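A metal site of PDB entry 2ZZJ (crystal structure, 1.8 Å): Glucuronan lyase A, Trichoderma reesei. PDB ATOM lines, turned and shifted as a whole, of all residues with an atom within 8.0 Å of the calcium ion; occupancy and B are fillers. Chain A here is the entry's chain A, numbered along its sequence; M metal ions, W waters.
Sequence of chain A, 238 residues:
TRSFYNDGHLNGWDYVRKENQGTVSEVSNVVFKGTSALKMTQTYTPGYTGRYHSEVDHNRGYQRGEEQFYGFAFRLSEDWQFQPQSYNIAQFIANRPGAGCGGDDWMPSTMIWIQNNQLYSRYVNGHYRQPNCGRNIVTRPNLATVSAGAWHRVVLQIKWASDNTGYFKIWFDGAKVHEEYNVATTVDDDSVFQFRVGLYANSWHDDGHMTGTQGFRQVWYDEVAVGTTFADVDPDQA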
ATOM      1  N   TYR A   5     -20.443 -11.689 -26.493  1.00  0.00           N
ATOM      2  CA  TYR A   5     -20.306 -12.830 -25.583  1.00  0.00           C
ATOM      3  C   TYR A   5     -21.140 -12.560 -24.357  1.00  0.00           C
ATOM      4  O   TYR A   5     -21.075 -11.444 -23.772  1.00  0.00           O
ATOM      5  CB  TYR A   5     -18.843 -13.095 -25.189  1.00  0.00           C
ATOM      6  CG  TYR A   5     -18.720 -14.117 -24.091  1.00  0.00           C
ATOM      7  CD1 TYR A   5     -19.130 -15.459 -24.287  1.00  0.00           C
ATOM      8  CD2 TYR A   5     -18.192 -13.761 -22.827  1.00  0.00           C
ATOM      9  CE1 TYR A   5     -19.038 -16.410 -23.244  1.00  0.00           C
ATOM     10  CE2 TYR A   5     -18.112 -14.701 -21.779  1.00  0.00           C
ATOM     11  CZ  TYR A   5     -18.507 -16.017 -21.998  1.00  0.00           C
ATOM     12  OH  TYR A   5     -18.418 -16.955 -20.989  1.00  0.00           O
ATOM     13  N   ASN A   6     -21.938 -13.539 -23.962  1.00  0.00           N
ATOM     14  CA  ASN A   6     -22.666 -13.414 -22.689  1.00  0.00           C
ATOM     15  C   ASN A   6     -22.558 -14.690 -21.876  1.00  0.00           C
ATOM     16  O   ASN A   6     -22.941 -15.775 -22.353  1.00  0.00           O
ATOM     17  CB  ASN A   6     -24.135 -13.057 -22.912  1.00  0.00           C
ATOM     18  CG  ASN A   6     -24.867 -12.770 -21.600  1.00  0.00           C
ATOM     19  OD1 ASN A   6     -25.422 -13.666 -20.960  1.00  0.00           O
ATOM     20  ND2 ASN A   6     -24.902 -11.474 -21.202  1.00  0.00           N
ATOM     21  N   ASP A   7     -22.063 -14.558 -20.638  1.00  0.00           N
ATOM     22  CA  ASP A   7     -21.822 -15.737 -19.793  1.00  0.00           C
ATOM     23  C   ASP A   7     -23.013 -16.100 -18.900  1.00  0.00           C
ATOM     24  O   ASP A   7     -22.826 -16.759 -17.858  1.00  0.00           O
ATOM     25  CB  ASP A   7     -20.609 -15.507 -18.880  1.00  0.00           C
ATOM     26  CG  ASP A   7     -20.868 -14.432 -17.823  1.00  0.00           C
ATOM     27  OD1 ASP A   7     -21.839 -13.653 -17.986  1.00  0.00           O
ATOM     28  OD2 ASP A   7     -20.084 -14.358 -16.838  1.00  0.00           O
ATOM     29  N   GLY A   8     -24.220 -15.747 -19.303  1.00  0.00           N
ATOM     30  CA  GLY A   8     -25.416 -16.122 -18.513  1.00  0.00           C
ATOM     31  C   GLY A   8     -25.738 -15.065 -17.464  1.00  0.00           C
ATOM     32  O   GLY A   8     -25.999 -15.400 -16.319  1.00  0.00           O
ATOM     33  N   HIS A   9     -25.757 -13.804 -17.897  1.00  0.00           N
ATOM     34  CA  HIS A   9     -26.103 -12.650 -17.065  1.00  0.00           C
ATOM     35  C   HIS A   9     -27.021 -11.682 -17.825  1.00  0.00           C
ATOM     36  O   HIS A   9     -27.008 -11.597 -19.068  1.00  0.00           O
ATOM     37  CB  HIS A   9     -24.829 -11.895 -16.661  1.00  0.00           C
ATOM     38  CG  HIS A   9     -24.117 -12.475 -15.471  1.00  0.00           C
ATOM     39  ND1 HIS A   9     -22.914 -13.138 -15.578  1.00  0.00           N
ATOM     40  CD2 HIS A   9     -24.443 -12.485 -14.150  1.00  0.00           C
ATOM     41  CE1 HIS A   9     -22.528 -13.530 -14.376  1.00  0.00           C
ATOM     42  NE2 HIS A   9     -23.452 -13.156 -13.496  1.00  0.00           N
ATOM     43  N   VAL A  27     -29.764 -17.175 -12.422  1.00  0.00           N
ATOM     44  CA  VAL A  27     -29.733 -18.233 -11.420  1.00  0.00           C
ATOM     45  C   VAL A  27     -28.305 -18.736 -11.277  1.00  0.00           C
ATOM     46  O   VAL A  27     -27.487 -18.524 -12.177  1.00  0.00           O
ATOM     47  CB  VAL A  27     -30.690 -19.405 -11.809  1.00  0.00           C
ATOM     48  CG1 VAL A  27     -32.137 -18.893 -11.976  1.00  0.00           C
ATOM     49  CG2 VAL A  27     -30.209 -20.137 -13.117  1.00  0.00           C
ATOM     50  N   VAL A  30     -28.513 -23.857 -11.676  1.00  0.00           N
ATOM     51  CA  VAL A  30     -28.581 -24.640 -12.902  1.00  0.00           C
ATOM     52  C   VAL A  30     -27.781 -23.818 -13.901  1.00  0.00           C
ATOM     53  O   VAL A  30     -28.245 -22.794 -14.371  1.00  0.00           O
ATOM     54  CB  VAL A  30     -30.046 -24.804 -13.394  1.00  0.00           C
ATOM     55  CG1 VAL A  30     -30.086 -25.582 -14.723  1.00  0.00           C
ATOM     56  CG2 VAL A  30     -30.930 -25.508 -12.308  1.00  0.00           C
ATOM     57  N   VAL A  31     -26.540 -24.238 -14.131  1.00  0.00           N
ATOM     58  CA  VAL A  31     -25.547 -23.411 -14.844  1.00  0.00           C
ATOM     59  C   VAL A  31     -24.742 -24.299 -15.789  1.00  0.00           C
ATOM     60  O   VAL A  31     -24.384 -25.415 -15.420  1.00  0.00           O
ATOM     61  CB  VAL A  31     -24.616 -22.692 -13.830  1.00  0.00           C
ATOM     62  CG1 VAL A  31     -23.396 -22.117 -14.523  1.00  0.00           C
ATOM     63  CG2 VAL A  31     -25.375 -21.598 -13.083  1.00  0.00           C
ATOM     64  N   PHE A  32     -24.449 -23.817 -16.993  1.00  0.00           N
ATOM     65  CA  PHE A  32     -23.607 -24.575 -17.887  1.00  0.00           C
ATOM     66  C   PHE A  32     -22.096 -24.353 -17.615  1.00  0.00           C
ATOM     67  O   PHE A  32     -21.318 -25.315 -17.572  1.00  0.00           O
ATOM     68  CB  PHE A  32     -23.954 -24.283 -19.363  1.00  0.00           C
ATOM     69  CG  PHE A  32     -23.039 -24.971 -20.342  1.00  0.00           C
ATOM     70  CD1 PHE A  32     -23.039 -26.378 -20.451  1.00  0.00           C
ATOM     71  CD2 PHE A  32     -22.172 -24.227 -21.146  1.00  0.00           C
ATOM     72  CE1 PHE A  32     -22.179 -27.036 -21.334  1.00  0.00           C
ATOM     73  CE2 PHE A  32     -21.295 -24.880 -22.057  1.00  0.00           C
ATOM     74  CZ  PHE A  32     -21.298 -26.295 -22.137  1.00  0.00           C
ATOM     75  N   LYS A  33     -21.695 -23.110 -17.452  1.00  0.00           N
ATOM     76  CA  LYS A  33     -20.281 -22.762 -17.238  1.00  0.00           C
ATOM     77  C   LYS A  33     -20.255 -21.587 -16.269  1.00  0.00           C
ATOM     78  O   LYS A  33     -21.175 -20.753 -16.298  1.00  0.00           O
ATOM     79  CB  LYS A  33     -19.617 -22.400 -18.581  1.00  0.00           C
ATOM     80  CG  LYS A  33     -18.106 -22.281 -18.549  1.00  0.00           C
ATOM     81  CD  LYS A  33     -17.501 -21.803 -19.896  1.00  0.00           C
ATOM     82  CE  LYS A  33     -17.808 -22.769 -21.071  1.00  0.00           C
ATOM     83  NZ  LYS A  33     -17.135 -22.397 -22.397  1.00  0.00           N
ATOM     84  N   GLY A  34     -19.214 -21.504 -15.430  1.00  0.00           N
ATOM     85  CA  GLY A  34     -19.144 -20.390 -14.475  1.00  0.00           C
ATOM     86  C   GLY A  34     -20.185 -20.528 -13.383  1.00  0.00           C
ATOM     87  O   GLY A  34     -20.554 -21.637 -13.027  1.00  0.00           O
ATOM     88  N   THR A  35     -20.697 -19.423 -12.869  1.00  0.00           N
ATOM     89  CA  THR A  35     -21.566 -19.473 -11.690  1.00  0.00           C
ATOM     90  C   THR A  35     -22.932 -18.860 -11.954  1.00  0.00           C
ATOM     91  O   THR A  35     -23.706 -18.604 -11.025  1.00  0.00           O
ATOM     92  CB  THR A  35     -20.919 -18.719 -10.498  1.00  0.00           C
ATOM     93  OG1 THR A  35     -20.704 -17.352 -10.853  1.00  0.00           O
ATOM     94  CG2 THR A  35     -19.592 -19.325 -10.143  1.00  0.00           C
ATOM     95  N   SER A  36     -23.246 -18.596 -13.226  1.00  0.00           N
ATOM     96  CA  SER A  36     -24.475 -17.917 -13.554  1.00  0.00           C
ATOM     97  C   SER A  36     -25.047 -18.476 -14.834  1.00  0.00           C
ATOM     98  O   SER A  36     -24.299 -18.857 -15.738  1.00  0.00           O
ATOM     99  CB  SER A  36     -24.194 -16.431 -13.747  1.00  0.00           C
ATOM    100  OG  SER A  36     -25.409 -15.716 -13.712  1.00  0.00           O
ATOM    101  N   ALA A  37     -26.371 -18.530 -14.911  1.00  0.00           N
ATOM    102  CA  ALA A  37     -27.057 -18.761 -16.195  1.00  0.00           C
ATOM    103  C   ALA A  37     -28.373 -17.987 -16.193  1.00  0.00           C
ATOM    104  O   ALA A  37     -28.741 -17.406 -15.161  1.00  0.00           O
ATOM    105  CB  ALA A  37     -27.286 -20.229 -16.410  1.00  0.00           C
ATOM    106  N   LEU A  38     -29.108 -18.006 -17.304  1.00  0.00           N
ATOM    107  CA  LEU A  38     -30.397 -17.344 -17.381  1.00  0.00           C
ATOM    108  C   LEU A  38     -31.486 -18.366 -17.396  1.00  0.00           C
ATOM    109  O   LEU A  38     -31.339 -19.381 -18.066  1.00  0.00           O
ATOM    110  CB  LEU A  38     -30.495 -16.482 -18.631  1.00  0.00           C
ATOM    111  CG  LEU A  38     -29.522 -15.296 -18.669  1.00  0.00           C
ATOM    112  CD1 LEU A  38     -29.599 -14.570 -20.014  1.00  0.00           C
ATOM    113  CD2 LEU A  38     -29.801 -14.312 -17.513  1.00  0.00           C
ATOM    114  N   TRP A 151     -27.895 -29.935 -20.405  1.00  0.00           N
ATOM    115  CA  TRP A 151     -27.399 -28.811 -21.225  1.00  0.00           C
ATOM    116  C   TRP A 151     -27.038 -29.287 -22.629  1.00  0.00           C
ATOM    117  O   TRP A 151     -26.225 -30.230 -22.799  1.00  0.00           O
ATOM    118  CB  TRP A 151     -26.173 -28.152 -20.602  1.00  0.00           C
ATOM    119  CG  TRP A 151     -26.534 -27.287 -19.430  1.00  0.00           C
ATOM    120  CD1 TRP A 151     -26.457 -27.608 -18.092  1.00  0.00           C
ATOM    121  CD2 TRP A 151     -27.063 -25.983 -19.503  1.00  0.00           C
ATOM    122  NE1 TRP A 151     -26.886 -26.539 -17.342  1.00  0.00           N
ATOM    123  CE2 TRP A 151     -27.265 -25.531 -18.184  1.00  0.00           C
ATOM    124  CE3 TRP A 151     -27.399 -25.139 -20.583  1.00  0.00           C
ATOM    125  CZ2 TRP A 151     -27.781 -24.258 -17.904  1.00  0.00           C
ATOM    126  CZ3 TRP A 151     -27.906 -23.885 -20.314  1.00  0.00           C
ATOM    127  CH2 TRP A 151     -28.099 -23.452 -18.971  1.00  0.00           C
ATOM    128  N   TYR A 221     -30.524 -20.861 -20.284  1.00  0.00           N
ATOM    129  CA  TYR A 221     -29.578 -20.513 -21.326  1.00  0.00           C
ATOM    130  C   TYR A 221     -28.267 -20.095 -20.707  1.00  0.00           C
ATOM    131  O   TYR A 221     -28.239 -19.576 -19.588  1.00  0.00           O
ATOM    132  CB  TYR A 221     -30.087 -19.321 -22.142  1.00  0.00           C
ATOM    133  CG  TYR A 221     -31.282 -19.640 -22.989  1.00  0.00           C
ATOM    134  CD1 TYR A 221     -31.112 -19.991 -24.334  1.00  0.00           C
ATOM    135  CD2 TYR A 221     -32.562 -19.612 -22.459  1.00  0.00           C
ATOM    136  CE1 TYR A 221     -32.247 -20.299 -25.162  1.00  0.00           C
ATOM    137  CE2 TYR A 221     -33.702 -19.936 -23.263  1.00  0.00           C
ATOM    138  CZ  TYR A 221     -33.509 -20.250 -24.596  1.00  0.00           C
ATOM    139  OH  TYR A 221     -34.645 -20.491 -25.344  1.00  0.00           O
ATOM    140  N   ASP A 222     -27.204 -20.243 -21.475  1.00  0.00           N
ATOM    141  CA  ASP A 222     -25.886 -19.798 -21.018  1.00  0.00           C
ATOM    142  C   ASP A 222     -24.937 -19.696 -22.206  1.00  0.00           C
ATOM    143  O   ASP A 222     -25.219 -20.255 -23.277  1.00  0.00           O
ATOM    144  CB  ASP A 222     -25.367 -20.827 -20.013  1.00  0.00           C
ATOM    145  CG  ASP A 222     -24.280 -20.257 -19.082  1.00  0.00           C
ATOM    146  OD1 ASP A 222     -23.852 -19.082 -19.253  1.00  0.00           O
ATOM    147  OD2 ASP A 222     -23.869 -21.012 -18.186  1.00  0.00           O
ATOM    148  N   GLU A 223     -23.795 -19.036 -21.996  1.00  0.00           N
ATOM    149  CA  GLU A 223     -22.690 -19.102 -22.892  1.00  0.00           C
ATOM    150  C   GLU A 223     -23.111 -18.778 -24.354  1.00  0.00           C
ATOM    151  O   GLU A 223     -22.960 -19.614 -25.240  1.00  0.00           O
ATOM    152  CB  GLU A 223     -22.021 -20.504 -22.759  1.00  0.00           C
ATOM    153  CG  GLU A 223     -20.592 -20.598 -23.224  1.00  0.00           C
ATOM    154  CD  GLU A 223     -19.581 -19.816 -22.340  1.00  0.00           C
ATOM    155  OE1 GLU A 223     -18.400 -19.890 -22.723  1.00  0.00           O
ATOM    156  OE2 GLU A 223     -19.944 -19.132 -21.333  1.00  0.00           O
ATOM    157  N   VAL A 224     -23.645 -17.575 -24.564  1.00  0.00           N
ATOM    158  CA  VAL A 224     -24.088 -17.144 -25.890  1.00  0.00           C
ATOM    159  C   VAL A 224     -22.991 -16.293 -26.513  1.00  0.00           C
ATOM    160  O   VAL A 224     -22.371 -15.472 -25.808  1.00  0.00           O
ATOM    161  CB  VAL A 224     -25.405 -16.301 -25.809  1.00  0.00           C
ATOM    162  CG1 VAL A 224     -25.963 -16.023 -27.236  1.00  0.00           C
ATOM    163  CG2 VAL A 224     -26.488 -17.024 -24.951  1.00  0.00           C
HETATM  164 CA    CA M   1     -22.461 -19.049 -17.242  1.00  0.00          CA
HETATM  165  O   HOH W   1     -21.377 -17.497 -15.624  1.00  0.00           O
HETATM  166  O   HOH W   2     -20.573 -18.985 -18.737  1.00  0.00           O
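The side-chain hydroxyl (OG) of Ser 36 lies within hydrogen-bond range of the backbone carbonyl oxygen (O) of Gly 8, at 2.7 Å. A ring nitrogen (NE2) of His 9 sits at hydrogen-bond distance from the side-chain hydroxyl (OG) of Ser 36 (3.2 Å). The side-chain carboxylate (OD2) of Asp 222 lies close to the backbone NH (N) of Phe 32 (3.1 Å). OD1 of Asp 7 lies within hydrogen-bond range of ND1 of His 9 (2.7 Å). The backbone NH of Gly 8 sits close to the side-chain carboxylate of Asp 222, 3.4 Å away. The side-chain amino group (NZ) of Lys 33 lies within salt-bridge range of the side-chain carboxylate (OE1) of Glu 223, 2.8 Å away.
Four residues have an atom within 4 Å of the calcium ion: Asp 7, Lys 33, Ser 36 and Asp 222. The nearest printed residue that does not touch the calcium ion is Val 31 (4.2 Å).
The calcium ion is bound by O of Lys 33 (2.3 Å), O of Ser 36 (2.4 Å), O of Asp 7 (2.4 Å), water W2 (2.4 Å), OD1 of Asp 222 (2.4 Å), water W1 (2.5 Å) and OD2 of Asp 222 (2.6 Å).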
